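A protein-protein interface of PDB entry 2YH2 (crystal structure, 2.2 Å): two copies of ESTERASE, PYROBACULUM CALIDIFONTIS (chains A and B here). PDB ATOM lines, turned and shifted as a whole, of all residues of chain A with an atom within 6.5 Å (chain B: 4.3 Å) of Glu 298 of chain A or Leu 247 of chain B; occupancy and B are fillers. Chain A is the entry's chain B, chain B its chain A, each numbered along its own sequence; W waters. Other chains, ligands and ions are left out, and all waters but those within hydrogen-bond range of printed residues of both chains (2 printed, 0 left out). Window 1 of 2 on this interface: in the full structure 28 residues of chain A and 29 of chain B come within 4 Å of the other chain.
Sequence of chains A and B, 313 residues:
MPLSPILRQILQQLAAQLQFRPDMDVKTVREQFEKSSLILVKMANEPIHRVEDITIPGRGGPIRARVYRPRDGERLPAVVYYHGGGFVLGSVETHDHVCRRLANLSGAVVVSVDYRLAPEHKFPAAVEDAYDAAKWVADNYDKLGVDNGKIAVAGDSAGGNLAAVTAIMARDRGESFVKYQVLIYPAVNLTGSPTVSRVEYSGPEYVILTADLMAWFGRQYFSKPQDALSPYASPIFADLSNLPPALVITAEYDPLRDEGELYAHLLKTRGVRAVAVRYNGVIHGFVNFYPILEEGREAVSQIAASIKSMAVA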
ATOM      1  N   TYR A 279      11.924   7.489 -23.624  1.00  0.00           N
ATOM      2  CA  TYR A 279      11.125   7.817 -24.815  1.00  0.00           C
ATOM      3  C   TYR A 279      10.017   6.770 -25.053  1.00  0.00           C
ATOM      4  O   TYR A 279      10.285   5.581 -25.287  1.00  0.00           O
ATOM      5  CB  TYR A 279      12.020   7.963 -26.049  1.00  0.00           C
ATOM      6  CG  TYR A 279      12.710   9.329 -26.137  1.00  0.00           C
ATOM      7  CD1 TYR A 279      13.667   9.711 -25.200  1.00  0.00           C
ATOM      8  CD2 TYR A 279      12.406  10.226 -27.168  1.00  0.00           C
ATOM      9  CE1 TYR A 279      14.291  10.959 -25.280  1.00  0.00           C
ATOM     10  CE2 TYR A 279      13.006  11.450 -27.252  1.00  0.00           C
ATOM     11  CZ  TYR A 279      13.943  11.827 -26.303  1.00  0.00           C
ATOM     12  OH  TYR A 279      14.553  13.067 -26.400  1.00  0.00           O
ATOM     13  N   TYR A 290      15.904   8.554 -36.937  1.00  0.00           N
ATOM     14  CA  TYR A 290      15.361   9.913 -36.790  1.00  0.00           C
ATOM     15  C   TYR A 290      14.835  10.568 -38.086  1.00  0.00           C
ATOM     16  O   TYR A 290      13.950  11.413 -38.011  1.00  0.00           O
ATOM     17  CB  TYR A 290      16.351  10.845 -36.071  1.00  0.00           C
ATOM     18  CG  TYR A 290      17.526  11.315 -36.885  1.00  0.00           C
ATOM     19  CD1 TYR A 290      17.383  12.314 -37.865  1.00  0.00           C
ATOM     20  CD2 TYR A 290      18.795  10.801 -36.661  1.00  0.00           C
ATOM     21  CE1 TYR A 290      18.471  12.745 -38.625  1.00  0.00           C
ATOM     22  CE2 TYR A 290      19.894  11.238 -37.410  1.00  0.00           C
ATOM     23  CZ  TYR A 290      19.730  12.197 -38.383  1.00  0.00           C
ATOM     24  OH  TYR A 290      20.840  12.620 -39.093  1.00  0.00           O
ATOM     25  N   LEU A 293      11.326   9.078 -37.663  1.00  0.00           N
ATOM     26  CA  LEU A 293      10.685   9.015 -36.358  1.00  0.00           C
ATOM     27  C   LEU A 293      10.932  10.315 -35.617  1.00  0.00           C
ATOM     28  O   LEU A 293      12.073  10.637 -35.325  1.00  0.00           O
ATOM     29  CB  LEU A 293      11.248   7.871 -35.504  1.00  0.00           C
ATOM     30  CG  LEU A 293      10.874   6.404 -35.690  1.00  0.00           C
ATOM     31  CD1 LEU A 293      11.508   5.605 -34.518  1.00  0.00           C
ATOM     32  CD2 LEU A 293       9.363   6.169 -35.753  1.00  0.00           C
ATOM     33  N   GLU A 294       9.867  11.031 -35.266  1.00  0.00           N
ATOM     34  CA  GLU A 294      10.007  12.286 -34.518  1.00  0.00           C
ATOM     35  C   GLU A 294      10.754  12.071 -33.190  1.00  0.00           C
ATOM     36  O   GLU A 294      11.569  12.905 -32.799  1.00  0.00           O
ATOM     37  CB  GLU A 294       8.646  13.003 -34.314  1.00  0.00           C
ATOM     38  CG  GLU A 294       7.588  12.245 -33.505  1.00  0.00           C
ATOM     39  CD  GLU A 294       6.651  11.443 -34.381  1.00  0.00           C
ATOM     40  OE1 GLU A 294       7.139  10.778 -35.312  1.00  0.00           O
ATOM     41  OE2 GLU A 294       5.426  11.492 -34.161  1.00  0.00           O
ATOM     42  N   GLU A 295      10.511  10.943 -32.525  1.00  0.00           N
ATOM     43  CA  GLU A 295      11.254  10.580 -31.298  1.00  0.00           C
ATOM     44  C   GLU A 295      12.758  10.626 -31.520  1.00  0.00           C
ATOM     45  O   GLU A 295      13.529  11.073 -30.658  1.00  0.00           O
ATOM     46  CB  GLU A 295      10.895   9.163 -30.840  1.00  0.00           C
ATOM     47  CG  GLU A 295       9.551   9.022 -30.170  1.00  0.00           C
ATOM     48  CD  GLU A 295       8.394   8.939 -31.127  1.00  0.00           C
ATOM     49  OE1 GLU A 295       8.600   8.940 -32.368  1.00  0.00           O
ATOM     50  OE2 GLU A 295       7.262   8.892 -30.627  1.00  0.00           O
ATOM     51  N   GLY A 296      13.180  10.144 -32.687  1.00  0.00           N
ATOM     52  CA  GLY A 296      14.598  10.178 -33.056  1.00  0.00           C
ATOM     53  C   GLY A 296      15.152  11.592 -33.098  1.00  0.00           C
ATOM     54  O   GLY A 296      16.198  11.877 -32.515  1.00  0.00           O
ATOM     55  N   ARG A 297      14.443  12.482 -33.783  1.00  0.00           N
ATOM     56  CA  ARG A 297      14.899  13.868 -33.924  1.00  0.00           C
ATOM     57  C   ARG A 297      14.921  14.545 -32.565  1.00  0.00           C
ATOM     58  O   ARG A 297      15.870  15.254 -32.231  1.00  0.00           O
ATOM     59  CB  ARG A 297      14.002  14.631 -34.883  1.00  0.00           C
ATOM     60  CG  ARG A 297      14.083  14.087 -36.303  1.00  0.00           C
ATOM     61  CD  ARG A 297      13.493  15.022 -37.319  1.00  0.00           C
ATOM     62  NE  ARG A 297      12.034  15.096 -37.258  1.00  0.00           N
ATOM     63  CZ  ARG A 297      11.187  14.132 -37.637  1.00  0.00           C
ATOM     64  NH1 ARG A 297      11.637  12.956 -38.089  1.00  0.00           N
ATOM     65  NH2 ARG A 297       9.868  14.343 -37.556  1.00  0.00           N
ATOM     66  N   GLU A 298      13.894  14.293 -31.764  1.00  0.00           N
ATOM     67  CA  GLU A 298      13.849  14.853 -30.417  1.00  0.00           C
ATOM     68  C   GLU A 298      15.054  14.379 -29.568  1.00  0.00           C
ATOM     69  O   GLU A 298      15.670  15.161 -28.852  1.00  0.00           O
ATOM     70  CB  GLU A 298      12.504  14.516 -29.755  1.00  0.00           C
ATOM     71  CG  GLU A 298      12.275  15.130 -28.386  1.00  0.00           C
ATOM     72  CD  GLU A 298      12.513  16.619 -28.355  1.00  0.00           C
ATOM     73  OE1 GLU A 298      12.079  17.303 -29.311  1.00  0.00           O
ATOM     74  OE2 GLU A 298      13.130  17.100 -27.367  1.00  0.00           O
ATOM     75  N   ALA A 299      15.404  13.107 -29.684  1.00  0.00           N
ATOM     76  CA  ALA A 299      16.525  12.543 -28.953  1.00  0.00           C
ATOM     77  C   ALA A 299      17.842  13.211 -29.321  1.00  0.00           C
ATOM     78  O   ALA A 299      18.635  13.577 -28.440  1.00  0.00           O
ATOM     79  CB  ALA A 299      16.610  11.063 -29.196  1.00  0.00           C
ATOM     80  N   VAL A 300      18.107  13.344 -30.615  1.00  0.00           N
ATOM     81  CA  VAL A 300      19.340  14.004 -31.030  1.00  0.00           C
ATOM     82  C   VAL A 300      19.378  15.459 -30.510  1.00  0.00           C
ATOM     83  O   VAL A 300      20.405  15.918 -30.004  1.00  0.00           O
ATOM     84  CB  VAL A 300      19.561  13.930 -32.542  1.00  0.00           C
ATOM     85  CG1 VAL A 300      20.863  14.660 -32.918  1.00  0.00           C
ATOM     86  CG2 VAL A 300      19.580  12.450 -33.009  1.00  0.00           C
ATOM     87  N   SER A 301      18.247  16.148 -30.595  1.00  0.00           N
ATOM     88  CA  SER A 301      18.111  17.510 -30.066  1.00  0.00           C
ATOM     89  C   SER A 301      18.434  17.539 -28.589  1.00  0.00           C
ATOM     90  O   SER A 301      19.197  18.394 -28.115  1.00  0.00           O
ATOM     91  CB  SER A 301      16.693  18.050 -30.312  1.00  0.00           C
ATOM     92  OG  SER A 301      16.431  19.246 -29.586  1.00  0.00           O
ATOM     93  N   GLN A 302      17.857  16.598 -27.860  1.00  0.00           N
ATOM     94  CA  GLN A 302      18.044  16.542 -26.431  1.00  0.00           C
ATOM     95  C   GLN A 302      19.490  16.247 -26.085  1.00  0.00           C
ATOM     96  O   GLN A 302      20.090  16.941 -25.264  1.00  0.00           O
ATOM     97  CB  GLN A 302      17.145  15.487 -25.788  1.00  0.00           C
ATOM     98  CG  GLN A 302      17.504  15.298 -24.328  1.00  0.00           C
ATOM     99  CD  GLN A 302      16.573  14.411 -23.556  1.00  0.00           C
ATOM    100  OE1 GLN A 302      15.870  13.566 -24.119  1.00  0.00           O
ATOM    101  NE2 GLN A 302      16.565  14.592 -22.236  1.00  0.00           N
ATOM    102  N   ILE A 303      20.025  15.202 -26.704  1.00  0.00           N
ATOM    103  CA  ILE A 303      21.409  14.784 -26.513  1.00  0.00           C
ATOM    104  C   ILE A 303      22.396  15.946 -26.760  1.00  0.00           C
ATOM    105  O   ILE A 303      23.225  16.260 -25.906  1.00  0.00           O
ATOM    106  CB  ILE A 303      21.763  13.546 -27.424  1.00  0.00           C
ATOM    107  CG1 ILE A 303      21.083  12.268 -26.907  1.00  0.00           C
ATOM    108  CG2 ILE A 303      23.264  13.303 -27.477  1.00  0.00           C
ATOM    109  CD1 ILE A 303      20.991  11.139 -27.943  1.00  0.00           C
ATOM    110  N   TYR B 180       4.084  25.023 -32.674  1.00  0.00           N
ATOM    111  CA  TYR B 180       4.753  24.027 -31.847  1.00  0.00           C
ATOM    112  C   TYR B 180       4.187  24.098 -30.449  1.00  0.00           C
ATOM    113  O   TYR B 180       3.841  25.177 -29.958  1.00  0.00           O
ATOM    114  CB  TYR B 180       6.253  24.336 -31.813  1.00  0.00           C
ATOM    115  CG  TYR B 180       7.178  23.168 -31.569  1.00  0.00           C
ATOM    116  CD1 TYR B 180       7.452  22.242 -32.576  1.00  0.00           C
ATOM    117  CD2 TYR B 180       7.824  23.013 -30.342  1.00  0.00           C
ATOM    118  CE1 TYR B 180       8.339  21.179 -32.349  1.00  0.00           C
ATOM    119  CE2 TYR B 180       8.689  21.965 -30.106  1.00  0.00           C
ATOM    120  CZ  TYR B 180       8.955  21.054 -31.108  1.00  0.00           C
ATOM    121  OH  TYR B 180       9.823  20.016 -30.854  1.00  0.00           O
ATOM    122  N   GLN B 181       4.067  22.951 -29.799  1.00  0.00           N
ATOM    123  CA  GLN B 181       3.523  22.927 -28.458  1.00  0.00           C
ATOM    124  C   GLN B 181       4.362  22.051 -27.557  1.00  0.00           C
ATOM    125  O   GLN B 181       4.747  20.952 -27.935  1.00  0.00           O
ATOM    126  CB  GLN B 181       2.058  22.497 -28.455  1.00  0.00           C
ATOM    127  CG  GLN B 181       1.766  21.080 -28.793  1.00  0.00           C
ATOM    128  CD  GLN B 181       0.280  20.849 -28.918  1.00  0.00           C
ATOM    129  OE1 GLN B 181      -0.488  21.100 -27.985  1.00  0.00           O
ATOM    130  NE2 GLN B 181      -0.141  20.399 -30.083  1.00  0.00           N
ATOM    131  N   VAL B 182       4.684  22.580 -26.380  1.00  0.00           N
ATOM    132  CA  VAL B 182       5.454  21.858 -25.397  1.00  0.00           C
ATOM    133  C   VAL B 182       4.581  21.809 -24.155  1.00  0.00           C
ATOM    134  O   VAL B 182       4.243  22.841 -23.594  1.00  0.00           O
ATOM    135  CB  VAL B 182       6.779  22.558 -25.094  1.00  0.00           C
ATOM    136  CG1 VAL B 182       7.454  21.901 -23.927  1.00  0.00           C
ATOM    137  CG2 VAL B 182       7.716  22.571 -26.352  1.00  0.00           C
ATOM    138  N   LEU B 183       4.188  20.611 -23.759  1.00  0.00           N
ATOM    139  CA  LEU B 183       3.267  20.408 -22.640  1.00  0.00           C
ATOM    140  C   LEU B 183       4.048  19.757 -21.490  1.00  0.00           C
ATOM    141  O   LEU B 183       4.453  18.589 -21.571  1.00  0.00           O
ATOM    142  CB  LEU B 183       2.075  19.538 -23.091  1.00  0.00           C
ATOM    143  CG  LEU B 183       1.316  20.029 -24.344  1.00  0.00           C
ATOM    144  CD1 LEU B 183       0.128  19.108 -24.726  1.00  0.00           C
ATOM    145  CD2 LEU B 183       0.822  21.453 -24.181  1.00  0.00           C
ATOM    146  N   ALA B 246       4.076  18.289 -31.197  1.00  0.00           N
ATOM    147  CA  ALA B 246       4.082  18.372 -29.741  1.00  0.00           C
ATOM    148  C   ALA B 246       5.234  17.634 -29.071  1.00  0.00           C
ATOM    149  O   ALA B 246       5.552  16.509 -29.439  1.00  0.00           O
ATOM    150  CB  ALA B 246       2.735  17.841 -29.186  1.00  0.00           C
ATOM    151  N   LEU B 247       5.833  18.273 -28.066  1.00  0.00           N
ATOM    152  CA  LEU B 247       6.677  17.587 -27.082  1.00  0.00           C
ATOM    153  C   LEU B 247       5.901  17.552 -25.774  1.00  0.00           C
ATOM    154  O   LEU B 247       5.457  18.597 -25.284  1.00  0.00           O
ATOM    155  CB  LEU B 247       8.027  18.304 -26.882  1.00  0.00           C
ATOM    156  CG  LEU B 247       8.974  17.720 -25.806  1.00  0.00           C
ATOM    157  CD1 LEU B 247       9.376  16.275 -26.104  1.00  0.00           C
ATOM    158  CD2 LEU B 247      10.198  18.580 -25.647  1.00  0.00           C
ATOM    159  N   VAL B 248       5.714  16.353 -25.220  1.00  0.00           N
ATOM    160  CA  VAL B 248       5.050  16.189 -23.919  1.00  0.00           C
ATOM    161  C   VAL B 248       6.027  15.614 -22.914  1.00  0.00           C
ATOM    162  O   VAL B 248       6.585  14.557 -23.138  1.00  0.00           O
ATOM    163  CB  VAL B 248       3.835  15.251 -24.020  1.00  0.00           C
ATOM    164  CG1 VAL B 248       3.145  15.105 -22.662  1.00  0.00           C
ATOM    165  CG2 VAL B 248       2.859  15.788 -25.092  1.00  0.00           C
ATOM    166  N   ILE B 249       6.249  16.327 -21.820  1.00  0.00           N
ATOM    167  CA  ILE B 249       7.155  15.878 -20.787  1.00  0.00           C
ATOM    168  C   ILE B 249       6.317  15.348 -19.636  1.00  0.00           C
ATOM    169  O   ILE B 249       5.417  16.038 -19.166  1.00  0.00           O
ATOM    170  CB  ILE B 249       8.012  17.017 -20.212  1.00  0.00           C
ATOM    171  CG1 ILE B 249       8.828  17.727 -21.305  1.00  0.00           C
ATOM    172  CG2 ILE B 249       8.930  16.468 -19.125  1.00  0.00           C
ATOM    173  CD1 ILE B 249       9.892  16.885 -21.944  1.00  0.00           C
ATOM    174  N   VAL B 275       5.970  13.562 -29.466  1.00  0.00           N
ATOM    175  CA  VAL B 275       6.883  12.748 -28.673  1.00  0.00           C
ATOM    176  C   VAL B 275       6.544  12.937 -27.198  1.00  0.00           C
ATOM    177  O   VAL B 275       6.341  14.057 -26.743  1.00  0.00           O
ATOM    178  CB  VAL B 275       8.351  13.169 -28.932  1.00  0.00           C
ATOM    179  CG1 VAL B 275       9.324  12.418 -27.992  1.00  0.00           C
ATOM    180  CG2 VAL B 275       8.726  12.953 -30.426  1.00  0.00           C
ATOM    181  N   GLN B 302      16.252  20.412 -22.674  1.00  0.00           N
ATOM    182  CA  GLN B 302      15.536  19.683 -23.709  1.00  0.00           C
ATOM    183  C   GLN B 302      14.437  20.520 -24.340  1.00  0.00           C
ATOM    184  O   GLN B 302      14.313  20.563 -25.558  1.00  0.00           O
ATOM    185  CB  GLN B 302      14.925  18.384 -23.179  1.00  0.00           C
ATOM    186  CG  GLN B 302      14.232  17.571 -24.273  1.00  0.00           C
ATOM    187  CD  GLN B 302      13.510  16.331 -23.779  1.00  0.00           C
ATOM    188  OE1 GLN B 302      13.514  16.012 -22.593  1.00  0.00           O
ATOM    189  NE2 GLN B 302      12.883  15.628 -24.701  1.00  0.00           N
ATOM    190  N   SER B 306      14.353  21.868 -28.170  1.00  0.00           N
ATOM    191  CA  SER B 306      13.243  21.345 -28.959  1.00  0.00           C
ATOM    192  C   SER B 306      12.499  22.483 -29.621  1.00  0.00           C
ATOM    193  O   SER B 306      12.217  22.407 -30.812  1.00  0.00           O
ATOM    194  CB  SER B 306      12.306  20.495 -28.115  1.00  0.00           C
ATOM    195  OG  SER B 306      11.363  19.841 -28.938  1.00  0.00           O
ATOM    196  N   ALA B 311      12.232  20.349 -33.134  1.00  0.00           N
ATOM    197  CA  ALA B 311      12.801  19.029 -33.373  1.00  0.00           C
ATOM    198  C   ALA B 311      11.730  17.991 -33.718  1.00  0.00           C
ATOM    199  O   ALA B 311      11.941  17.181 -34.609  1.00  0.00           O
ATOM    200  CB  ALA B 311      13.628  18.584 -32.162  1.00  0.00           C
ATOM    201  N   VAL B 312      10.569  18.054 -33.056  1.00  0.00           N
ATOM    202  CA  VAL B 312       9.490  17.090 -33.293  1.00  0.00           C
ATOM    203  C   VAL B 312       8.814  17.246 -34.677  1.00  0.00           C
ATOM    204  O   VAL B 312       8.279  16.270 -35.218  1.00  0.00           O
ATOM    205  CB  VAL B 312       8.449  17.132 -32.146  1.00  0.00           C
ATOM    206  CG1 VAL B 312       7.231  16.248 -32.442  1.00  0.00           C
ATOM    207  CG2 VAL B 312       9.086  16.730 -30.829  1.00  0.00           C
HETATM  208  O   HOH W   1      18.876  18.372 -23.278  1.00  0.00           O
HETATM  209  O   HOH W   2      15.374  18.682 -27.312  1.00  0.00           O
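NE2 of Gln 302 of chain B is in hydrogen-bond range of OH of Tyr 279 of chain A (3.5 Å).
OE2 of Glu 298 of chain A is in hydrogen-bond range of NE2 of Gln 302 of chain B, at 3.1 Å.
The side-chain amide nitrogen of Gln 302 of chain A lies within hydrogen-bond range of the side-chain amide oxygen of Gln 302 of chain B (3.4 Å).
The side-chain carboxylate of Glu 298 of chain A lies within hydrogen-bond range of the side-chain hydroxyl of Ser 306 of chain B (2.7 Å).
O of Ala 311 of chain B sits close to NE of Arg 297 of chain A.
The backbone carbonyl oxygen (O) of Val 312 of chain B sits at hydrogen-bond distance from the guanidinium group (NH2) of Arg 297 of chain A.
The side-chain hydroxyl (OH) of Tyr 180 of chain B lies within hydrogen-bond range of the backbone NH (N) of Val 312 of chain B (3.0 Å).
The backbone carbonyl oxygen of Ala 246 of chain B lies within hydrogen-bond range of the backbone NH of Val 275 of chain B (3.0 Å).
O of Ser 306 of chain B sits at hydrogen-bond distance from N of Ala 311 of chain B, at 3.1 Å.
OH of Tyr 279 of chain A sits close to N of Ala 299 of chain A (3.4 Å).
The side-chain hydroxyl (OH) of Tyr 279 of chain A sits at hydrogen-bond distance from the side-chain amide oxygen (OE1) of Gln 302 of chain A (2.7 Å).
The backbone carbonyl oxygen (O) of Tyr 290 of chain A is in hydrogen-bond range of the guanidinium group (NH1) of Arg 297 of chain A (2.8 Å).
CD2 of Tyr 279 of chain A touches CG1 of Val 275 of chain B, at 3.9 Å.
CG of Glu 294 of chain A touches CG2 of Val 275 of chain B (3.4 Å).
O of Val 312 of chain B touches CB of Glu 294 of chain A, at 3.4 Å.
Val 275 of chain B touches Glu 295 of chain A.
Tyr 180 of chain B touches Glu 298 of chain A (OH to OE1, 3.9 Å).
CD2 of Leu 247 of chain B touches OE2 of Glu 298 of chain A, 3.7 Å away.
Ala 311 of chain B touches Glu 298 of chain A (CB to OE1, 3.5 Å).
CG2 of Val 312 of chain B touches OE1 of Glu 298 of chain A, 3.4 Å away.
OG of Ser 301 of chain A touches N of Ser 306 of chain B (3.6 Å).
CB of Ala 311 of chain B touches CB of Ser 301 of chain A, 3.6 Å away.
Printed residues of chain B within 4 Å of Tyr 279 of chain A: Val 275 (3.9 Å) and Gln 302 (3.5 Å).
Glu 298 of chain A touches just these residues of chain B: Tyr 180 (3.9 Å), Leu 247 (3.7 Å), Gln 302 (3.1 Å), Ser 306 (2.7 Å), Ala 311 (3.5 Å) and Val 312 (3.4 Å).
Ala 299 of chain A touches none of the printed residues of chain B.
Of the printed residues of chain B, Gln 302 of chain A touches Gln 302.
Of chain A, only Glu 298 comes within 4 Å of Leu 247 of chain B.
Printed residues of chain B that touch a printed residue of chain A: Tyr 180, Leu 247, Val 275, Gln 302, Ser 306, Ala 311 and Val 312.
Hydrophobic or aromatic side chains of chain B that line the printed part of chain A: Tyr 180, Leu 247, Val 275, Ala 311 and Val 312.
Along chain B the printed residues that touch a printed residue of chain A span positions 180 to 312.
Printed residues of chain A that touch a printed residue of chain B: Tyr 279, Glu 294, Glu 295, Arg 297, Glu 298, Ser 301 and Gln 302.
Among the printed residues, no Asp or Glu carboxylate lies within 4 Å of a Lys or Arg side-chain nitrogen of the other chain.
Gln 302 of chain A touches its own counterpart, Gln 302 of chain B.
Position printed for both chains: 302.
Of the 16 pairs that touch across the chains among the printed residues, 1 has its exchanged pair printed and touching as well.
Water W2 lies within hydrogen-bond range of OG of Ser 301 of chain A, OE2 of Glu 298 of chain A, O of Gln 302 of chain B, N of Gln 302 of chain A and N of Ser 306 of chain B.
Water W1 bridges O of Gln 302 of chain A and N of Gln 302 of chain B.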
